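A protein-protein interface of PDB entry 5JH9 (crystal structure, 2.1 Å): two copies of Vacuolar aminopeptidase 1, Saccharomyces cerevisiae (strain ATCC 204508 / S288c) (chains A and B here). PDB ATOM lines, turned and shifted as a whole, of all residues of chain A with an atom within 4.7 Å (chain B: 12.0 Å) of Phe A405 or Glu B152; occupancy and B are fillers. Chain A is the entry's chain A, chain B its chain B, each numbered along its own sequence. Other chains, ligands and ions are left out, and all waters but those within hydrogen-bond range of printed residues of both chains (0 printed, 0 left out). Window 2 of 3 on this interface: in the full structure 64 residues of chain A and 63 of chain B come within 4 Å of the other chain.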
ATOM      1  N   TYR A 392     -19.557  22.772   0.410  1.00  0.00           N
ATOM      2  CA  TYR A 392     -20.685  22.068   1.006  1.00  0.00           C
ATOM      3  C   TYR A 392     -21.607  23.077   1.682  1.00  0.00           C
ATOM      4  O   TYR A 392     -21.150  23.907   2.461  1.00  0.00           O
ATOM      5  CB  TYR A 392     -20.180  21.065   2.042  1.00  0.00           C
ATOM      6  CG  TYR A 392     -21.249  20.205   2.684  1.00  0.00           C
ATOM      7  CD1 TYR A 392     -21.830  19.147   1.986  1.00  0.00           C
ATOM      8  CD2 TYR A 392     -21.664  20.436   3.994  1.00  0.00           C
ATOM      9  CE1 TYR A 392     -22.794  18.347   2.570  1.00  0.00           C
ATOM     10  CE2 TYR A 392     -22.629  19.637   4.595  1.00  0.00           C
ATOM     11  CZ  TYR A 392     -23.194  18.597   3.877  1.00  0.00           C
ATOM     12  OH  TYR A 392     -24.148  17.806   4.468  1.00  0.00           O
ATOM     13  N   TYR A 400     -24.943  17.309  -2.574  1.00  0.00           N
ATOM     14  CA  TYR A 400     -23.495  17.160  -2.462  1.00  0.00           C
ATOM     15  C   TYR A 400     -23.115  15.686  -2.392  1.00  0.00           C
ATOM     16  O   TYR A 400     -23.763  14.892  -1.693  1.00  0.00           O
ATOM     17  CB  TYR A 400     -22.968  17.947  -1.263  1.00  0.00           C
ATOM     18  CG  TYR A 400     -22.990  19.430  -1.534  1.00  0.00           C
ATOM     19  CD1 TYR A 400     -21.920  20.057  -2.178  1.00  0.00           C
ATOM     20  CD2 TYR A 400     -24.095  20.199  -1.202  1.00  0.00           C
ATOM     21  CE1 TYR A 400     -21.943  21.418  -2.447  1.00  0.00           C
ATOM     22  CE2 TYR A 400     -24.132  21.560  -1.475  1.00  0.00           C
ATOM     23  CZ  TYR A 400     -23.052  22.166  -2.090  1.00  0.00           C
ATOM     24  OH  TYR A 400     -23.085  23.514  -2.355  1.00  0.00           O
ATOM     25  N   LEU A 401     -22.078  15.332  -3.143  1.00  0.00           N
ATOM     26  CA  LEU A 401     -21.603  13.957  -3.220  1.00  0.00           C
ATOM     27  C   LEU A 401     -20.705  13.641  -2.026  1.00  0.00           C
ATOM     28  O   LEU A 401     -19.687  14.303  -1.830  1.00  0.00           O
ATOM     29  CB  LEU A 401     -20.831  13.745  -4.523  1.00  0.00           C
ATOM     30  CG  LEU A 401     -20.244  12.348  -4.769  1.00  0.00           C
ATOM     31  CD1 LEU A 401     -21.326  11.276  -4.741  1.00  0.00           C
ATOM     32  CD2 LEU A 401     -19.476  12.316  -6.083  1.00  0.00           C
ATOM     33  N   LYS A 402     -21.074  12.618  -1.253  1.00  0.00           N
ATOM     34  CA  LYS A 402     -20.287  12.178  -0.092  1.00  0.00           C
ATOM     35  C   LYS A 402     -18.856  11.845  -0.516  1.00  0.00           C
ATOM     36  O   LYS A 402     -18.643  11.242  -1.569  1.00  0.00           O
ATOM     37  CB  LYS A 402     -20.935  10.957   0.587  1.00  0.00           C
ATOM     38  CG  LYS A 402     -20.197  10.464   1.830  1.00  0.00           C
ATOM     39  CD  LYS A 402     -20.944   9.354   2.556  1.00  0.00           C
ATOM     40  CE  LYS A 402     -20.142   8.870   3.759  1.00  0.00           C
ATOM     41  NZ  LYS A 402     -20.891   7.897   4.603  1.00  0.00           N
ATOM     42  N   ASN A 403     -17.895  12.279   0.303  1.00  0.00           N
ATOM     43  CA  ASN A 403     -16.454  12.173   0.022  1.00  0.00           C
ATOM     44  C   ASN A 403     -15.937  13.028  -1.138  1.00  0.00           C
ATOM     45  O   ASN A 403     -14.754  12.946  -1.467  1.00  0.00           O
ATOM     46  CB  ASN A 403     -16.022  10.710  -0.166  1.00  0.00           C
ATOM     47  CG  ASN A 403     -16.435   9.832   0.997  1.00  0.00           C
ATOM     48  OD1 ASN A 403     -16.266  10.215   2.149  1.00  0.00           O
ATOM     49  ND2 ASN A 403     -16.973   8.652   0.701  1.00  0.00           N
ATOM     50  N   HIS A 404     -16.799  13.852  -1.737  1.00  0.00           N
ATOM     51  CA  HIS A 404     -16.426  14.686  -2.879  1.00  0.00           C
ATOM     52  C   HIS A 404     -17.001  16.092  -2.728  1.00  0.00           C
ATOM     53  O   HIS A 404     -17.530  16.644  -3.687  1.00  0.00           O
ATOM     54  CB  HIS A 404     -16.922  14.081  -4.197  1.00  0.00           C
ATOM     55  CG  HIS A 404     -16.453  12.688  -4.454  1.00  0.00           C
ATOM     56  ND1 HIS A 404     -16.968  11.594  -3.791  1.00  0.00           N
ATOM     57  CD2 HIS A 404     -15.549  12.203  -5.339  1.00  0.00           C
ATOM     58  CE1 HIS A 404     -16.383  10.498  -4.239  1.00  0.00           C
ATOM     59  NE2 HIS A 404     -15.521  10.839  -5.180  1.00  0.00           N
ATOM     60  N   PHE A 405     -16.908  16.661  -1.527  1.00  0.00           N
ATOM     61  CA  PHE A 405     -17.200  18.081  -1.319  1.00  0.00           C
ATOM     62  C   PHE A 405     -16.110  18.725  -0.474  1.00  0.00           C
ATOM     63  O   PHE A 405     -15.545  18.072   0.397  1.00  0.00           O
ATOM     64  CB  PHE A 405     -18.591  18.324  -0.700  1.00  0.00           C
ATOM     65  CG  PHE A 405     -18.835  17.618   0.615  1.00  0.00           C
ATOM     66  CD1 PHE A 405     -18.335  18.128   1.812  1.00  0.00           C
ATOM     67  CD2 PHE A 405     -19.616  16.470   0.663  1.00  0.00           C
ATOM     68  CE1 PHE A 405     -18.574  17.484   3.021  1.00  0.00           C
ATOM     69  CE2 PHE A 405     -19.870  15.825   1.872  1.00  0.00           C
ATOM     70  CZ  PHE A 405     -19.344  16.330   3.052  1.00  0.00           C
ATOM     71  N   PRO A 406     -15.798  20.004  -0.744  1.00  0.00           N
ATOM     72  CA  PRO A 406     -14.867  20.744   0.093  1.00  0.00           C
ATOM     73  C   PRO A 406     -15.548  21.472   1.253  1.00  0.00           C
ATOM     74  O   PRO A 406     -16.756  21.730   1.212  1.00  0.00           O
ATOM     75  CB  PRO A 406     -14.283  21.759  -0.881  1.00  0.00           C
ATOM     76  CG  PRO A 406     -15.427  22.087  -1.776  1.00  0.00           C
ATOM     77  CD  PRO A 406     -16.219  20.804  -1.911  1.00  0.00           C
ATOM     78  N   VAL A 407     -14.747  21.818   2.257  1.00  0.00           N
ATOM     79  CA  VAL A 407     -15.193  22.597   3.413  1.00  0.00           C
ATOM     80  C   VAL A 407     -14.295  23.834   3.546  1.00  0.00           C
ATOM     81  O   VAL A 407     -13.219  23.871   2.940  1.00  0.00           O
ATOM     82  CB  VAL A 407     -15.198  21.746   4.704  1.00  0.00           C
ATOM     83  CG1 VAL A 407     -16.225  20.624   4.591  1.00  0.00           C
ATOM     84  CG2 VAL A 407     -13.824  21.165   5.018  1.00  0.00           C
ATOM     85  N   GLN A 444      -8.662  19.214  -1.627  1.00  0.00           N
ATOM     86  CA  GLN A 444     -10.023  18.696  -1.473  1.00  0.00           C
ATOM     87  C   GLN A 444     -10.563  18.295  -2.842  1.00  0.00           C
ATOM     88  O   GLN A 444      -9.972  18.623  -3.877  1.00  0.00           O
ATOM     89  CB  GLN A 444     -10.931  19.752  -0.829  1.00  0.00           C
ATOM     90  CG  GLN A 444     -10.301  20.480   0.348  1.00  0.00           C
ATOM     91  CD  GLN A 444     -11.302  21.298   1.140  1.00  0.00           C
ATOM     92  OE1 GLN A 444     -12.067  20.751   1.928  1.00  0.00           O
ATOM     93  NE2 GLN A 444     -11.286  22.620   0.952  1.00  0.00           N
ATOM     94  N   TYR A 445     -11.687  17.585  -2.836  1.00  0.00           N
ATOM     95  CA  TYR A 445     -12.366  17.147  -4.056  1.00  0.00           C
ATOM     96  C   TYR A 445     -13.751  17.785  -4.185  1.00  0.00           C
ATOM     97  O   TYR A 445     -14.454  17.993  -3.178  1.00  0.00           O
ATOM     98  CB  TYR A 445     -12.555  15.627  -4.039  1.00  0.00           C
ATOM     99  CG  TYR A 445     -11.325  14.761  -4.224  1.00  0.00           C
ATOM    100  CD1 TYR A 445     -10.089  15.284  -4.636  1.00  0.00           C
ATOM    101  CD2 TYR A 445     -11.420  13.382  -4.042  1.00  0.00           C
ATOM    102  CE1 TYR A 445      -8.992  14.462  -4.818  1.00  0.00           C
ATOM    103  CE2 TYR A 445     -10.326  12.555  -4.227  1.00  0.00           C
ATOM    104  CZ  TYR A 445      -9.115  13.099  -4.616  1.00  0.00           C
ATOM    105  OH  TYR A 445      -8.037  12.272  -4.794  1.00  0.00           O
ATOM    106  N   LYS B 148     -27.768  23.236  17.490  1.00  0.00           N
ATOM    107  CA  LYS B 148     -27.787  22.226  16.440  1.00  0.00           C
ATOM    108  C   LYS B 148     -26.469  21.475  16.481  1.00  0.00           C
ATOM    109  O   LYS B 148     -25.432  22.054  16.825  1.00  0.00           O
ATOM    110  CB  LYS B 148     -27.980  22.878  15.074  1.00  0.00           C
ATOM    111  CG  LYS B 148     -29.346  23.521  14.903  1.00  0.00           C
ATOM    112  CD  LYS B 148     -29.594  23.997  13.482  1.00  0.00           C
ATOM    113  CE  LYS B 148     -29.985  22.858  12.547  1.00  0.00           C
ATOM    114  NZ  LYS B 148     -31.341  22.305  12.811  1.00  0.00           N
ATOM    115  N   ASP B 149     -26.519  20.181  16.163  1.00  0.00           N
ATOM    116  CA  ASP B 149     -25.310  19.376  16.001  1.00  0.00           C
ATOM    117  C   ASP B 149     -24.537  19.914  14.798  1.00  0.00           C
ATOM    118  O   ASP B 149     -25.144  20.410  13.849  1.00  0.00           O
ATOM    119  CB  ASP B 149     -25.653  17.898  15.744  1.00  0.00           C
ATOM    120  CG  ASP B 149     -26.281  17.202  16.950  1.00  0.00           C
ATOM    121  OD1 ASP B 149     -25.930  17.522  18.106  1.00  0.00           O
ATOM    122  OD2 ASP B 149     -27.120  16.304  16.734  1.00  0.00           O
ATOM    123  N   THR B 150     -23.211  19.829  14.836  1.00  0.00           N
ATOM    124  CA  THR B 150     -22.406  20.247  13.693  1.00  0.00           C
ATOM    125  C   THR B 150     -22.721  19.345  12.501  1.00  0.00           C
ATOM    126  O   THR B 150     -22.943  18.146  12.660  1.00  0.00           O
ATOM    127  CB  THR B 150     -20.896  20.233  13.990  1.00  0.00           C
ATOM    128  OG1 THR B 150     -20.521  18.961  14.523  1.00  0.00           O
ATOM    129  CG2 THR B 150     -20.541  21.321  14.994  1.00  0.00           C
ATOM    130  N   ALA B 151     -22.777  19.951  11.318  1.00  0.00           N
ATOM    131  CA  ALA B 151     -23.152  19.266  10.085  1.00  0.00           C
ATOM    132  C   ALA B 151     -21.957  19.335   9.137  1.00  0.00           C
ATOM    133  O   ALA B 151     -21.732  20.364   8.491  1.00  0.00           O
ATOM    134  CB  ALA B 151     -24.377  19.931   9.471  1.00  0.00           C
ATOM    135  N   GLU B 152     -21.188  18.243   9.092  1.00  0.00           N
ATOM    136  CA  GLU B 152     -19.913  18.172   8.359  1.00  0.00           C
ATOM    137  C   GLU B 152     -18.950  19.307   8.758  1.00  0.00           C
ATOM    138  O   GLU B 152     -18.236  19.864   7.915  1.00  0.00           O
ATOM    139  CB  GLU B 152     -20.159  18.164   6.839  1.00  0.00           C
ATOM    140  CG  GLU B 152     -21.148  17.098   6.353  1.00  0.00           C
ATOM    141  CD  GLU B 152     -20.675  15.667   6.569  1.00  0.00           C
ATOM    142  OE1 GLU B 152     -19.452  15.426   6.629  1.00  0.00           O
ATOM    143  OE2 GLU B 152     -21.537  14.768   6.664  1.00  0.00           O
ATOM    144  N   GLY B 153     -18.949  19.650  10.047  1.00  0.00           N
ATOM    145  CA  GLY B 153     -18.101  20.708  10.584  1.00  0.00           C
ATOM    146  C   GLY B 153     -18.726  22.092  10.667  1.00  0.00           C
ATOM    147  O   GLY B 153     -18.200  22.956  11.370  1.00  0.00           O
ATOM    148  N   TYR B 154     -19.829  22.323   9.956  1.00  0.00           N
ATOM    149  CA  TYR B 154     -20.516  23.619   9.998  1.00  0.00           C
ATOM    150  C   TYR B 154     -21.290  23.796  11.300  1.00  0.00           C
ATOM    151  O   TYR B 154     -22.023  22.902  11.724  1.00  0.00           O
ATOM    152  CB  TYR B 154     -21.494  23.778   8.833  1.00  0.00           C
ATOM    153  CG  TYR B 154     -20.861  24.136   7.514  1.00  0.00           C
ATOM    154  CD1 TYR B 154     -20.640  25.469   7.171  1.00  0.00           C
ATOM    155  CD2 TYR B 154     -20.504  23.156   6.601  1.00  0.00           C
ATOM    156  CE1 TYR B 154     -20.073  25.814   5.952  1.00  0.00           C
ATOM    157  CE2 TYR B 154     -19.936  23.492   5.381  1.00  0.00           C
ATOM    158  CZ  TYR B 154     -19.723  24.821   5.064  1.00  0.00           C
ATOM    159  OH  TYR B 154     -19.166  25.149   3.849  1.00  0.00           O
ATOM    160  N   GLY B 155     -21.112  24.958  11.918  1.00  0.00           N
ATOM    161  CA  GLY B 155     -21.942  25.401  13.021  1.00  0.00           C
ATOM    162  C   GLY B 155     -23.169  26.104  12.468  1.00  0.00           C
ATOM    163  O   GLY B 155     -23.048  26.967  11.592  1.00  0.00           O
ATOM    164  N   ARG B 156     -24.346  25.721  12.967  1.00  0.00           N
ATOM    165  CA  ARG B 156     -25.618  26.364  12.624  1.00  0.00           C
ATOM    166  C   ARG B 156     -26.411  26.642  13.898  1.00  0.00           C
ATOM    167  O   ARG B 156     -26.139  26.046  14.934  1.00  0.00           O
ATOM    168  CB  ARG B 156     -26.446  25.462  11.703  1.00  0.00           C
ATOM    169  CG  ARG B 156     -25.848  25.265  10.323  1.00  0.00           C
ATOM    170  CD  ARG B 156     -26.768  24.454   9.425  1.00  0.00           C
ATOM    171  NE  ARG B 156     -26.958  23.085   9.909  1.00  0.00           N
ATOM    172  CZ  ARG B 156     -27.750  22.181   9.340  1.00  0.00           C
ATOM    173  NH1 ARG B 156     -28.442  22.478   8.243  1.00  0.00           N
ATOM    174  NH2 ARG B 156     -27.853  20.963   9.873  1.00  0.00           N
ATOM    175  N   LEU B 209     -28.401  28.164  -2.276  1.00  0.00           N
ATOM    176  CA  LEU B 209     -27.771  27.106  -3.055  1.00  0.00           C
ATOM    177  C   LEU B 209     -27.444  27.646  -4.440  1.00  0.00           C
ATOM    178  O   LEU B 209     -28.254  28.350  -5.039  1.00  0.00           O
ATOM    179  CB  LEU B 209     -28.704  25.893  -3.175  1.00  0.00           C
ATOM    180  CG  LEU B 209     -28.142  24.660  -3.895  1.00  0.00           C
ATOM    181  CD1 LEU B 209     -26.900  24.148  -3.183  1.00  0.00           C
ATOM    182  CD2 LEU B 209     -29.201  23.570  -3.978  1.00  0.00           C
ATOM    183  N   PHE B 213     -26.834  23.574  -9.395  1.00  0.00           N
ATOM    184  CA  PHE B 213     -27.447  22.306  -8.966  1.00  0.00           C
ATOM    185  C   PHE B 213     -28.872  22.058  -9.497  1.00  0.00           C
ATOM    186  O   PHE B 213     -29.404  20.958  -9.337  1.00  0.00           O
ATOM    187  CB  PHE B 213     -27.399  22.198  -7.437  1.00  0.00           C
ATOM    188  CG  PHE B 213     -26.005  22.095  -6.900  1.00  0.00           C
ATOM    189  CD1 PHE B 213     -25.330  20.878  -6.929  1.00  0.00           C
ATOM    190  CD2 PHE B 213     -25.341  23.217  -6.413  1.00  0.00           C
ATOM    191  CE1 PHE B 213     -24.030  20.775  -6.457  1.00  0.00           C
ATOM    192  CE2 PHE B 213     -24.041  23.121  -5.941  1.00  0.00           C
ATOM    193  CZ  PHE B 213     -23.387  21.898  -5.960  1.00  0.00           C
ATOM    194  N   ILE B 228     -31.622  27.896   7.286  1.00  0.00           N
ATOM    195  CA  ILE B 228     -30.988  27.798   8.601  1.00  0.00           C
ATOM    196  C   ILE B 228     -29.697  28.629   8.585  1.00  0.00           C
ATOM    197  O   ILE B 228     -28.834  28.400   7.729  1.00  0.00           O
ATOM    198  CB  ILE B 228     -30.662  26.330   8.959  1.00  0.00           C
ATOM    199  CG1 ILE B 228     -31.939  25.464   8.904  1.00  0.00           C
ATOM    200  CG2 ILE B 228     -30.026  26.252  10.338  1.00  0.00           C
ATOM    201  CD1 ILE B 228     -31.684  23.973   8.878  1.00  0.00           C
ATOM    202  N   VAL B 230     -26.023  29.815   9.079  1.00  0.00           N
ATOM    203  CA  VAL B 230     -24.718  29.198   9.294  1.00  0.00           C
ATOM    204  C   VAL B 230     -23.880  30.178  10.107  1.00  0.00           C
ATOM    205  O   VAL B 230     -23.597  31.285   9.648  1.00  0.00           O
ATOM    206  CB  VAL B 230     -24.018  28.878   7.956  1.00  0.00           C
ATOM    207  CG1 VAL B 230     -22.594  28.385   8.182  1.00  0.00           C
ATOM    208  CG2 VAL B 230     -24.829  27.848   7.178  1.00  0.00           C
ATOM    209  N   ILE B 231     -23.476  29.757  11.303  1.00  0.00           N
ATOM    210  CA  ILE B 231     -22.824  30.638  12.263  1.00  0.00           C
ATOM    211  C   ILE B 231     -21.289  30.486  12.311  1.00  0.00           C
ATOM    212  O   ILE B 231     -20.589  31.438  12.679  1.00  0.00           O
ATOM    213  CB  ILE B 231     -23.493  30.492  13.661  1.00  0.00           C
ATOM    214  CG1 ILE B 231     -23.281  31.753  14.502  1.00  0.00           C
ATOM    215  CG2 ILE B 231     -23.018  29.243  14.403  1.00  0.00           C
ATOM    216  CD1 ILE B 231     -24.146  31.814  15.742  1.00  0.00           C
ATOM    217  N   GLY B 232     -20.763  29.324  11.922  1.00  0.00           N
ATOM    218  CA  GLY B 232     -19.312  29.109  11.917  1.00  0.00           C
ATOM    219  C   GLY B 232     -18.850  27.805  11.290  1.00  0.00           C
ATOM    220  O   GLY B 232     -19.662  27.000  10.829  1.00  0.00           O
ATOM    221  N   PHE B 233     -17.533  27.634  11.236  1.00  0.00           N
ATOM    222  CA  PHE B 233     -16.890  26.352  10.950  1.00  0.00           C
ATOM    223  C   PHE B 233     -15.677  26.197  11.886  1.00  0.00           C
ATOM    224  O   PHE B 233     -14.543  26.452  11.483  1.00  0.00           O
ATOM    225  CB  PHE B 233     -16.483  26.268   9.471  1.00  0.00           C
ATOM    226  CG  PHE B 233     -16.272  24.862   8.985  1.00  0.00           C
ATOM    227  CD1 PHE B 233     -15.053  24.216   9.174  1.00  0.00           C
ATOM    228  CD2 PHE B 233     -17.299  24.174   8.350  1.00  0.00           C
ATOM    229  CE1 PHE B 233     -14.866  22.915   8.733  1.00  0.00           C
ATOM    230  CE2 PHE B 233     -17.117  22.875   7.905  1.00  0.00           C
ATOM    231  CZ  PHE B 233     -15.900  22.243   8.101  1.00  0.00           C
ATOM    232  N   PRO B 234     -15.917  25.804  13.155  1.00  0.00           N
ATOM    233  CA  PRO B 234     -14.826  25.772  14.141  1.00  0.00           C
ATOM    234  C   PRO B 234     -13.773  24.689  13.890  1.00  0.00           C
ATOM    235  O   PRO B 234     -14.052  23.695  13.217  1.00  0.00           O
ATOM    236  CB  PRO B 234     -15.555  25.529  15.470  1.00  0.00           C
ATOM    237  CG  PRO B 234     -16.851  24.905  15.099  1.00  0.00           C
ATOM    238  CD  PRO B 234     -17.217  25.465  13.761  1.00  0.00           C
ATOM    239  N   THR B 235     -12.575  24.908  14.432  1.00  0.00           N
ATOM    240  CA  THR B 235     -11.448  23.975  14.320  1.00  0.00           C
ATOM    241  C   THR B 235     -10.977  23.538  15.709  1.00  0.00           C
ATOM    242  O   THR B 235     -11.282  24.208  16.701  1.00  0.00           O
ATOM    243  CB  THR B 235     -10.259  24.632  13.592  1.00  0.00           C
ATOM    244  OG1 THR B 235      -9.780  25.745  14.357  1.00  0.00           O
ATOM    245  CG2 THR B 235     -10.675  25.106  12.207  1.00  0.00           C
ATOM    246  N   PRO B 236     -10.225  22.418  15.789  1.00  0.00           N
ATOM    247  CA  PRO B 236      -9.640  22.000  17.068  1.00  0.00           C
ATOM    248  C   PRO B 236      -8.324  22.717  17.363  1.00  0.00           C
ATOM    249  O   PRO B 236      -8.332  23.864  17.811  1.00  0.00           O
ATOM    250  CB  PRO B 236      -9.405  20.503  16.865  1.00  0.00           C
ATOM    251  CG  PRO B 236      -9.155  20.363  15.404  1.00  0.00           C
ATOM    252  CD  PRO B 236      -9.967  21.429  14.723  1.00  0.00           C
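Of the printed residues of chain B, Tyr A392 touches Glu B152 and Tyr B154.
Of chain B, only Leu B209 (3.95 Å) and Phe B213 (3.7 Å) come within 4 Å of Tyr A400.
No residue of chain B comes within 4 Å of Lys A402.
No residue of chain B comes within 4 Å of Asn A403.
No residue of chain B comes within 4 Å of His A404.
Lys B148 touches none of the printed residues of chain A.
Of the printed residues of chain A, Glu B152 touches Tyr A392 (3.4 Å), Phe A405 (3.7 Å) and Val A407 (3.96 Å).
Gly B153 touches none of the printed residues of chain A.
Of the printed residues of chain A, Tyr B154 touches Tyr A392.
Of the printed residues of chain A, Leu B209 touches Tyr A400 (3.95 Å).
Of the printed residues of chain A, Phe B233 touches Val A407 (3.5 Å).
Printed residues of chain B that touch a printed residue of chain A: Glu B152, Tyr B154, Leu B209, Phe B213 and Phe B233.
Of the 11 printed residues of chain A, 4 touch a printed residue of chain B.
Printed residues of chain A that touch a printed residue of chain B: Tyr A392, Tyr A400, Phe A405 and Val A407.
Hydrophobic or aromatic side chains of chain A within 4 Å of the printed part of chain B: Tyr A392, Tyr A400, Phe A405 and Val A407.
Along chain A the printed residues that touch a printed residue of chain B span positions 392 to 407.
Among the printed residues, 7 pairs touch across the chains.
Among the printed residues, no Asp or Glu carboxylate lies within 4 Å of a Lys or Arg side-chain nitrogen of the other chain.
O of Pro A406 is in hydrogen-bond range of N of Tyr A392 (3.1 Å).
N of Phe A405 sits at hydrogen-bond distance from O of Tyr A445.
The backbone NH (N) of Val A407 sits at hydrogen-bond distance from the side-chain amide oxygen (OE1) of Gln A444, at 2.9 Å.
Among the printed residues, pairs that only touch across the chains: Tyr A392 with Glu B152 (3.4 Å), Tyr A400 with Leu B209 (3.95 Å), Tyr A400 with Phe B213 (3.7 Å), Phe A405 with Glu B152 (3.7 Å), Val A407 with Glu B152 (3.96 Å) and Val A407 with Phe B233 (3.5 Å).
O of Tyr A392 sits at hydrogen-bond distance from OH of Tyr B154 (2.7 Å).
No position is printed for both chains.
Of the 7 pairs that touch across the chains among the printed residues, none has its exchanged pair printed and touching as well.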
